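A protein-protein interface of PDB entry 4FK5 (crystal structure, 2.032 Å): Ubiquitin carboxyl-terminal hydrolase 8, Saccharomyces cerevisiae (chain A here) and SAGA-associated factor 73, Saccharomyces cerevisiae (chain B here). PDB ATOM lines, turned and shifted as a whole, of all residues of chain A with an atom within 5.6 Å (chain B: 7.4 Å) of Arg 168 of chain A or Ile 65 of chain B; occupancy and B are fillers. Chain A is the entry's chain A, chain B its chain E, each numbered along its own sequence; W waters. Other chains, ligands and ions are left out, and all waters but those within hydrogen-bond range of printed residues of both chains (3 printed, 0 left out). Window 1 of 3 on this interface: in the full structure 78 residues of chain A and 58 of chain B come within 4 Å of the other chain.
The side-chain hydroxyl (OH) of Tyr 165 of chain A sits at hydrogen-bond distance from the backbone NH (N) of Ile 65 of chain B, 2.9 Å away. The guanidinium group (NH2) of Arg 168 of chain A lies within hydrogen-bond range of the side-chain amide oxygen (OE1) of Gln 63 of chain B (2.8 Å). The backbone carbonyl oxygen of Met 171 of chain A is in hydrogen-bond range of the backbone NH of Ala 86 of chain B.
The backbone NH (N) of Tyr 165 of chain A lies within hydrogen-bond range of the side-chain amide oxygen (OD1) of Asn 163 of chain A, at 3.0 Å. OG of Ser 172 of chain A lies within hydrogen-bond range of O of Arg 168 of chain A. The side-chain amide oxygen (OE1) of Gln 173 of chain A lies close to the backbone carbonyl oxygen (O) of Met 171 of chain A (3.2 Å).
Among the printed residues, merely in contact across the chains: Pro 164 of chain A with Ile 65 of chain B, Pro 164 of chain A with Pro 68 of chain B, Tyr 165 of chain A with Gln 63 of chain B, Tyr 165 of chain A with Leu 64 of chain B, Arg 168 of chain A with Ile 65 of chain B, Met 171 of chain A with Ala 89 of chain B, Ser 172 of chain A with Ala 86 of chain B, Ser 172 of chain A with Ala 89 of chain B and Ile 472 of chain A with Leu 64 of chain B.
Of the printed residues of chain B, Pro 164 of chain A touches Ile 65 and Pro 68. Arg 168 of chain A touches just these residues of chain B: Gln 63 (2.8 Å) and Ile 65 (3.6 Å). Printed residues of chain A within 4 Å of Leu 64 of chain B: Tyr 165 and Ile 472. Of chain A, only Pro 164 (3.9 Å), Tyr 165 (2.9 Å) and Arg 168 (3.6 Å) come within 4 Å of Ile 65 of chain B. Printed residues of chain A within 4 Å of Ala 86 of chain B: Met 171 (3.0 Å) and Ser 172 (3.9 Å). The nearest residue of chain A that does not touch Ile 65 of chain B is Ile 472 of chain A (4.3 Å).
Printed residues of chain B that touch a printed residue of chain A: Gln 63, Leu 64, Ile 65, Pro 68, Ala 86 and Ala 89. Along chain B the printed residues that touch a printed residue of chain A span positions 63 to 89. Printed residues of chain A that touch a printed residue of chain B: Pro 164, Tyr 165, Arg 168, Met 171, Ser 172 and Ile 472. Hydrophobic or aromatic side chains of chain A within 4 Å of the printed part of chain B: Pro 164, Tyr 165, Met 171 and Ile 472.
Water W3 lies within hydrogen-bond range of the backbone carbonyl oxygen of Ile 472 of chain A, the side-chain hydroxyl of Tyr 165 of chain A and the backbone carbonyl oxygen of Ile 65 of chain B. Water W2 lies within hydrogen-bond range of N of Asp 67 of chain B (2.7 Å), O of Ile 472 of chain A (3.5 Å) and SD of Met 49 of chain B (3.7 Å). Water W1 bridges the guanidinium group of Arg 168 of chain A (3.0 Å) and the backbone NH of Leu 64 of chain B (3.2 Å).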
ATOM      1  N   ASN A 163      -5.940  -2.958  -6.263  1.00  0.00           N
ATOM      2  CA  ASN A 163      -6.591  -1.797  -5.781  1.00  0.00           C
ATOM      3  C   ASN A 163      -7.665  -1.418  -6.830  1.00  0.00           C
ATOM      4  O   ASN A 163      -7.328  -1.219  -8.001  1.00  0.00           O
ATOM      5  CB  ASN A 163      -5.578  -0.659  -5.584  1.00  0.00           C
ATOM      6  CG  ASN A 163      -6.237   0.635  -5.098  1.00  0.00           C
ATOM      7  OD1 ASN A 163      -6.922   1.353  -5.878  1.00  0.00           O
ATOM      8  ND2 ASN A 163      -6.142   0.883  -3.811  1.00  0.00           N
ATOM      9  N   PRO A 164      -8.935  -1.318  -6.414  1.00  0.00           N
ATOM     10  CA  PRO A 164     -10.064  -1.051  -7.385  1.00  0.00           C
ATOM     11  C   PRO A 164      -9.938   0.238  -8.226  1.00  0.00           C
ATOM     12  O   PRO A 164     -10.295   0.226  -9.413  1.00  0.00           O
ATOM     13  CB  PRO A 164     -11.310  -1.018  -6.485  1.00  0.00           C
ATOM     14  CG  PRO A 164     -10.811  -0.800  -5.093  1.00  0.00           C
ATOM     15  CD  PRO A 164      -9.422  -1.443  -5.021  1.00  0.00           C
ATOM     16  N   TYR A 165      -9.334   1.287  -7.645  1.00  0.00           N
ATOM     17  CA  TYR A 165      -9.141   2.529  -8.315  1.00  0.00           C
ATOM     18  C   TYR A 165      -8.044   2.435  -9.341  1.00  0.00           C
ATOM     19  O   TYR A 165      -8.178   2.943 -10.461  1.00  0.00           O
ATOM     20  CB  TYR A 165      -8.838   3.636  -7.301  1.00  0.00           C
ATOM     21  CG  TYR A 165     -10.020   3.990  -6.401  1.00  0.00           C
ATOM     22  CD1 TYR A 165     -10.221   3.331  -5.201  1.00  0.00           C
ATOM     23  CD2 TYR A 165     -10.891   4.998  -6.745  1.00  0.00           C
ATOM     24  CE1 TYR A 165     -11.290   3.672  -4.365  1.00  0.00           C
ATOM     25  CE2 TYR A 165     -11.987   5.327  -5.947  1.00  0.00           C
ATOM     26  CZ  TYR A 165     -12.206   4.632  -4.770  1.00  0.00           C
ATOM     27  OH  TYR A 165     -13.301   4.981  -3.934  1.00  0.00           O
ATOM     28  N   PHE A 166      -6.953   1.759  -9.014  1.00  0.00           N
ATOM     29  CA  PHE A 166      -5.879   1.636 -10.011  1.00  0.00           C
ATOM     30  C   PHE A 166      -6.292   0.720 -11.121  1.00  0.00           C
ATOM     31  O   PHE A 166      -5.948   0.937 -12.316  1.00  0.00           O
ATOM     32  CB  PHE A 166      -4.579   1.096  -9.389  1.00  0.00           C
ATOM     33  CG  PHE A 166      -3.461   1.076 -10.353  1.00  0.00           C
ATOM     34  CD1 PHE A 166      -2.915   2.274 -10.801  1.00  0.00           C
ATOM     35  CD2 PHE A 166      -3.098  -0.077 -10.956  1.00  0.00           C
ATOM     36  CE1 PHE A 166      -1.980   2.297 -11.813  1.00  0.00           C
ATOM     37  CE2 PHE A 166      -2.113  -0.084 -11.941  1.00  0.00           C
ATOM     38  CZ  PHE A 166      -1.576   1.116 -12.383  1.00  0.00           C
ATOM     39  N   ILE A 167      -6.958  -0.357 -10.772  1.00  0.00           N
ATOM     40  CA  ILE A 167      -7.364  -1.337 -11.791  1.00  0.00           C
ATOM     41  C   ILE A 167      -8.389  -0.728 -12.754  1.00  0.00           C
ATOM     42  O   ILE A 167      -8.276  -0.889 -13.966  1.00  0.00           O
ATOM     43  CB  ILE A 167      -7.894  -2.612 -11.174  1.00  0.00           C
ATOM     44  CG1 ILE A 167      -6.782  -3.304 -10.428  1.00  0.00           C
ATOM     45  CG2 ILE A 167      -8.308  -3.593 -12.269  1.00  0.00           C
ATOM     46  CD1 ILE A 167      -5.628  -3.743 -11.369  1.00  0.00           C
ATOM     47  N   ARG A 168      -9.335   0.030 -12.240  1.00  0.00           N
ATOM     48  CA  ARG A 168     -10.260   0.816 -13.113  1.00  0.00           C
ATOM     49  C   ARG A 168      -9.500   1.833 -14.012  1.00  0.00           C
ATOM     50  O   ARG A 168      -9.650   1.822 -15.229  1.00  0.00           O
ATOM     51  CB  ARG A 168     -11.351   1.556 -12.287  1.00  0.00           C
ATOM     52  CG  ARG A 168     -12.268   2.423 -13.159  1.00  0.00           C
ATOM     53  CD  ARG A 168     -13.416   3.000 -12.339  1.00  0.00           C
ATOM     54  NE  ARG A 168     -12.930   4.154 -11.604  1.00  0.00           N
ATOM     55  CZ  ARG A 168     -13.700   5.053 -11.021  1.00  0.00           C
ATOM     56  NH1 ARG A 168     -15.014   4.912 -11.060  1.00  0.00           N
ATOM     57  NH2 ARG A 168     -13.160   6.105 -10.414  1.00  0.00           N
ATOM     58  N   HIS A 169      -8.577   2.588 -13.427  1.00  0.00           N
ATOM     59  CA  HIS A 169      -7.714   3.458 -14.209  1.00  0.00           C
ATOM     60  C   HIS A 169      -6.964   2.769 -15.349  1.00  0.00           C
ATOM     61  O   HIS A 169      -7.014   3.208 -16.527  1.00  0.00           O
ATOM     62  CB  HIS A 169      -6.778   4.141 -13.298  1.00  0.00           C
ATOM     63  CG  HIS A 169      -5.793   5.042 -13.978  1.00  0.00           C
ATOM     64  ND1 HIS A 169      -6.102   6.281 -14.361  1.00  0.00           N
ATOM     65  CD2 HIS A 169      -4.450   4.891 -14.221  1.00  0.00           C
ATOM     66  CE1 HIS A 169      -5.008   6.875 -14.863  1.00  0.00           C
ATOM     67  NE2 HIS A 169      -4.021   6.026 -14.802  1.00  0.00           N
ATOM     68  N   SER A 170      -6.266   1.699 -15.042  1.00  0.00           N
ATOM     69  CA  SER A 170      -5.519   1.010 -16.024  1.00  0.00           C
ATOM     70  C   SER A 170      -6.413   0.400 -17.114  1.00  0.00           C
ATOM     71  O   SER A 170      -6.139   0.565 -18.325  1.00  0.00           O
ATOM     72  CB  SER A 170      -4.624  -0.070 -15.355  1.00  0.00           C
ATOM     73  OG  SER A 170      -3.879  -0.752 -16.356  1.00  0.00           O
ATOM     74  N   MET A 171      -7.463  -0.309 -16.714  1.00  0.00           N
ATOM     75  CA  MET A 171      -8.369  -0.945 -17.680  1.00  0.00           C
ATOM     76  C   MET A 171      -9.211   0.061 -18.504  1.00  0.00           C
ATOM     77  O   MET A 171      -9.755  -0.305 -19.592  1.00  0.00           O
ATOM     78  CB  MET A 171      -9.288  -1.923 -16.977  1.00  0.00           C
ATOM     79  CG  MET A 171      -8.554  -3.180 -16.495  1.00  0.00           C
ATOM     80  SD  MET A 171      -9.767  -4.485 -16.148  1.00  0.00           S
ATOM     81  CE  MET A 171      -8.736  -5.704 -15.352  1.00  0.00           C
ATOM     82  N   SER A 172      -9.356   1.302 -17.981  1.00  0.00           N
ATOM     83  CA  SER A 172      -9.964   2.367 -18.768  1.00  0.00           C
ATOM     84  C   SER A 172      -9.091   2.916 -19.875  1.00  0.00           C
ATOM     85  O   SER A 172      -9.546   3.741 -20.621  1.00  0.00           O
ATOM     86  CB  SER A 172     -10.417   3.496 -17.866  1.00  0.00           C
ATOM     87  OG  SER A 172     -11.352   2.962 -16.896  1.00  0.00           O
ATOM     88  N   GLN A 173      -7.842   2.450 -19.992  1.00  0.00           N
ATOM     89  CA  GLN A 173      -6.910   2.908 -21.066  1.00  0.00           C
ATOM     90  C   GLN A 173      -6.506   4.386 -21.033  1.00  0.00           C
ATOM     91  O   GLN A 173      -5.964   4.910 -22.028  1.00  0.00           O
ATOM     92  CB  GLN A 173      -7.480   2.610 -22.458  1.00  0.00           C
ATOM     93  CG  GLN A 173      -7.991   1.224 -22.624  1.00  0.00           C
ATOM     94  CD  GLN A 173      -6.958   0.184 -22.291  1.00  0.00           C
ATOM     95  OE1 GLN A 173      -7.164  -0.662 -21.392  1.00  0.00           O
ATOM     96  NE2 GLN A 173      -5.836   0.230 -22.985  1.00  0.00           N
ATOM     97  N   ILE A 472     -12.509   3.642   1.009  1.00  0.00           N
ATOM     98  CA  ILE A 472     -13.723   4.255   1.600  1.00  0.00           C
ATOM     99  C   ILE A 472     -14.956   3.364   1.279  1.00  0.00           C
ATOM    100  O   ILE A 472     -15.112   2.835   0.169  1.00  0.00           O
ATOM    101  CB  ILE A 472     -13.888   5.768   1.257  1.00  0.00           C
ATOM    102  CG1 ILE A 472     -14.990   6.416   2.157  1.00  0.00           C
ATOM    103  CG2 ILE A 472     -14.154   5.979  -0.284  1.00  0.00           C
ATOM    104  CD1 ILE A 472     -14.688   6.377   3.693  1.00  0.00           C
ATOM    105  N   TYR B  46     -24.747   8.565  -4.201  1.00  0.00           N
ATOM    106  CA  TYR B  46     -24.315   7.239  -3.646  1.00  0.00           C
ATOM    107  C   TYR B  46     -25.338   6.733  -2.650  1.00  0.00           C
ATOM    108  O   TYR B  46     -26.017   7.509  -2.001  1.00  0.00           O
ATOM    109  CB  TYR B  46     -22.936   7.366  -3.008  1.00  0.00           C
ATOM    110  CG  TYR B  46     -21.866   7.884  -4.041  1.00  0.00           C
ATOM    111  CD1 TYR B  46     -21.400   7.075  -5.075  1.00  0.00           C
ATOM    112  CD2 TYR B  46     -21.478   9.175  -4.023  1.00  0.00           C
ATOM    113  CE1 TYR B  46     -20.459   7.581  -6.022  1.00  0.00           C
ATOM    114  CE2 TYR B  46     -20.568   9.705  -4.926  1.00  0.00           C
ATOM    115  CZ  TYR B  46     -20.069   8.922  -5.922  1.00  0.00           C
ATOM    116  OH  TYR B  46     -19.201   9.515  -6.778  1.00  0.00           O
ATOM    117  N   MET B  49     -22.917   7.016   0.801  1.00  0.00           N
ATOM    118  CA  MET B  49     -21.865   8.001   0.982  1.00  0.00           C
ATOM    119  C   MET B  49     -22.541   9.376   0.817  1.00  0.00           C
ATOM    120  O   MET B  49     -22.896   9.802  -0.286  1.00  0.00           O
ATOM    121  CB  MET B  49     -20.701   7.786   0.011  1.00  0.00           C
ATOM    122  CG  MET B  49     -19.977   6.457   0.220  1.00  0.00           C
ATOM    123  SD  MET B  49     -18.378   6.296  -0.662  1.00  0.00           S
ATOM    124  CE  MET B  49     -19.000   6.250  -2.346  1.00  0.00           C
ATOM    125  N   ALA B  62     -12.323  14.153  -5.641  1.00  0.00           N
ATOM    126  CA  ALA B  62     -12.064  12.739  -5.270  1.00  0.00           C
ATOM    127  C   ALA B  62     -12.688  11.779  -6.262  1.00  0.00           C
ATOM    128  O   ALA B  62     -13.851  11.904  -6.603  1.00  0.00           O
ATOM    129  CB  ALA B  62     -12.589  12.448  -3.882  1.00  0.00           C
ATOM    130  N   GLN B  63     -11.946  10.762  -6.676  1.00  0.00           N
ATOM    131  CA  GLN B  63     -12.604   9.611  -7.296  1.00  0.00           C
ATOM    132  C   GLN B  63     -13.265   8.778  -6.238  1.00  0.00           C
ATOM    133  O   GLN B  63     -12.664   8.528  -5.180  1.00  0.00           O
ATOM    134  CB  GLN B  63     -11.613   8.714  -8.051  1.00  0.00           C
ATOM    135  CG  GLN B  63     -10.872   9.383  -9.135  1.00  0.00           C
ATOM    136  CD  GLN B  63     -10.253   8.377 -10.088  1.00  0.00           C
ATOM    137  OE1 GLN B  63     -10.646   7.227 -10.104  1.00  0.00           O
ATOM    138  NE2 GLN B  63      -9.381   8.840 -10.945  1.00  0.00           N
ATOM    139  N   LEU B  64     -14.465   8.257  -6.556  1.00  0.00           N
ATOM    140  CA  LEU B  64     -15.230   7.450  -5.610  1.00  0.00           C
ATOM    141  C   LEU B  64     -15.845   6.263  -6.265  1.00  0.00           C
ATOM    142  O   LEU B  64     -16.559   6.406  -7.262  1.00  0.00           O
ATOM    143  CB  LEU B  64     -16.336   8.280  -4.955  1.00  0.00           C
ATOM    144  CG  LEU B  64     -15.823   9.453  -4.077  1.00  0.00           C
ATOM    145  CD1 LEU B  64     -16.968  10.435  -3.769  1.00  0.00           C
ATOM    146  CD2 LEU B  64     -15.163   8.930  -2.785  1.00  0.00           C
ATOM    147  N   ILE B  65     -15.594   5.082  -5.706  1.00  0.00           N
ATOM    148  CA  ILE B  65     -16.266   3.857  -6.151  1.00  0.00           C
ATOM    149  C   ILE B  65     -16.992   3.329  -4.945  1.00  0.00           C
ATOM    150  O   ILE B  65     -16.382   3.061  -3.902  1.00  0.00           O
ATOM    151  CB  ILE B  65     -15.269   2.783  -6.629  1.00  0.00           C
ATOM    152  CG1 ILE B  65     -14.447   3.308  -7.844  1.00  0.00           C
ATOM    153  CG2 ILE B  65     -16.008   1.479  -6.996  1.00  0.00           C
ATOM    154  CD1 ILE B  65     -13.263   2.426  -8.206  1.00  0.00           C
ATOM    155  N   GLU B  66     -18.283   3.313  -5.012  1.00  0.00           N
ATOM    156  CA  GLU B  66     -19.053   2.768  -3.919  1.00  0.00           C
ATOM    157  C   GLU B  66     -18.995   1.255  -3.939  1.00  0.00           C
ATOM    158  O   GLU B  66     -19.205   0.618  -5.000  1.00  0.00           O
ATOM    159  CB  GLU B  66     -20.510   3.229  -4.009  1.00  0.00           C
ATOM    160  CG  GLU B  66     -21.276   2.830  -2.782  1.00  0.00           C
ATOM    161  CD  GLU B  66     -22.588   3.609  -2.640  1.00  0.00           C
ATOM    162  OE1 GLU B  66     -23.304   3.771  -3.665  1.00  0.00           O
ATOM    163  OE2 GLU B  66     -22.859   4.052  -1.521  1.00  0.00           O
ATOM    164  N   ASP B  67     -18.780   0.680  -2.764  1.00  0.00           N
ATOM    165  CA  ASP B  67     -18.704  -0.773  -2.566  1.00  0.00           C
ATOM    166  C   ASP B  67     -17.816  -1.437  -3.651  1.00  0.00           C
ATOM    167  O   ASP B  67     -18.302  -2.337  -4.379  1.00  0.00           O
ATOM    168  CB  ASP B  67     -20.090  -1.418  -2.574  1.00  0.00           C
ATOM    169  CG  ASP B  67     -21.012  -0.874  -1.472  1.00  0.00           C
ATOM    170  OD1 ASP B  67     -20.519  -0.385  -0.395  1.00  0.00           O
ATOM    171  OD2 ASP B  67     -22.235  -0.882  -1.723  1.00  0.00           O
ATOM    172  N   PRO B  68     -16.507  -1.050  -3.711  1.00  0.00           N
ATOM    173  CA  PRO B  68     -15.646  -1.484  -4.790  1.00  0.00           C
ATOM    174  C   PRO B  68     -15.430  -2.990  -4.812  1.00  0.00           C
ATOM    175  O   PRO B  68     -15.108  -3.534  -5.845  1.00  0.00           O
ATOM    176  CB  PRO B  68     -14.316  -0.730  -4.501  1.00  0.00           C
ATOM    177  CG  PRO B  68     -14.357  -0.480  -3.041  1.00  0.00           C
ATOM    178  CD  PRO B  68     -15.778  -0.249  -2.713  1.00  0.00           C
ATOM    179  N   LEU B  69     -15.600  -3.660  -3.680  1.00  0.00           N
ATOM    180  CA  LEU B  69     -15.461  -5.146  -3.635  1.00  0.00           C
ATOM    181  C   LEU B  69     -16.807  -5.885  -3.686  1.00  0.00           C
ATOM    182  O   LEU B  69     -16.882  -7.099  -3.417  1.00  0.00           O
ATOM    183  CB  LEU B  69     -14.704  -5.548  -2.390  1.00  0.00           C
ATOM    184  CG  LEU B  69     -13.178  -5.654  -2.517  1.00  0.00           C
ATOM    185  CD1 LEU B  69     -12.575  -4.383  -2.964  1.00  0.00           C
ATOM    186  CD2 LEU B  69     -12.584  -6.114  -1.188  1.00  0.00           C
ATOM    187  N   ILE B  73     -14.122  -7.517 -10.698  1.00  0.00           N
ATOM    188  CA  ILE B  73     -13.896  -6.507 -11.682  1.00  0.00           C
ATOM    189  C   ILE B  73     -14.628  -6.877 -12.999  1.00  0.00           C
ATOM    190  O   ILE B  73     -14.566  -8.025 -13.463  1.00  0.00           O
ATOM    191  CB  ILE B  73     -12.386  -6.263 -11.875  1.00  0.00           C
ATOM    192  CG1 ILE B  73     -12.132  -5.299 -13.021  1.00  0.00           C
ATOM    193  CG2 ILE B  73     -11.649  -7.558 -12.037  1.00  0.00           C
ATOM    194  CD1 ILE B  73     -12.647  -3.895 -12.766  1.00  0.00           C
ATOM    195  N   ALA B  86     -12.078  -2.124 -19.503  1.00  0.00           N
ATOM    196  CA  ALA B  86     -13.264  -1.664 -18.737  1.00  0.00           C
ATOM    197  C   ALA B  86     -14.458  -1.520 -19.685  1.00  0.00           C
ATOM    198  O   ALA B  86     -14.279  -1.204 -20.874  1.00  0.00           O
ATOM    199  CB  ALA B  86     -12.971  -0.332 -18.061  1.00  0.00           C
ATOM    200  N   THR B  88     -16.737   0.735 -20.147  1.00  0.00           N
ATOM    201  CA  THR B  88     -16.763   2.090 -20.761  1.00  0.00           C
ATOM    202  C   THR B  88     -15.548   2.411 -21.674  1.00  0.00           C
ATOM    203  O   THR B  88     -15.480   3.493 -22.239  1.00  0.00           O
ATOM    204  CB  THR B  88     -16.846   3.168 -19.679  1.00  0.00           C
ATOM    205  OG1 THR B  88     -15.874   2.883 -18.677  1.00  0.00           O
ATOM    206  CG2 THR B  88     -18.264   3.191 -19.006  1.00  0.00           C
ATOM    207  N   ALA B  89     -14.605   1.481 -21.835  1.00  0.00           N
ATOM    208  CA  ALA B  89     -13.456   1.716 -22.749  1.00  0.00           C
ATOM    209  C   ALA B  89     -13.485   0.845 -24.020  1.00  0.00           C
ATOM    210  O   ALA B  89     -12.616   0.966 -24.858  1.00  0.00           O
ATOM    211  CB  ALA B  89     -12.130   1.515 -22.023  1.00  0.00           C
HETATM  212  O   HOH W   1     -15.087   8.315  -9.644  1.00  0.00           O
HETATM  213  O   HOH W   2     -18.439   2.588  -0.879  1.00  0.00           O
HETATM  214  O   HOH W   3     -13.958   2.975  -2.243  1.00  0.00           O
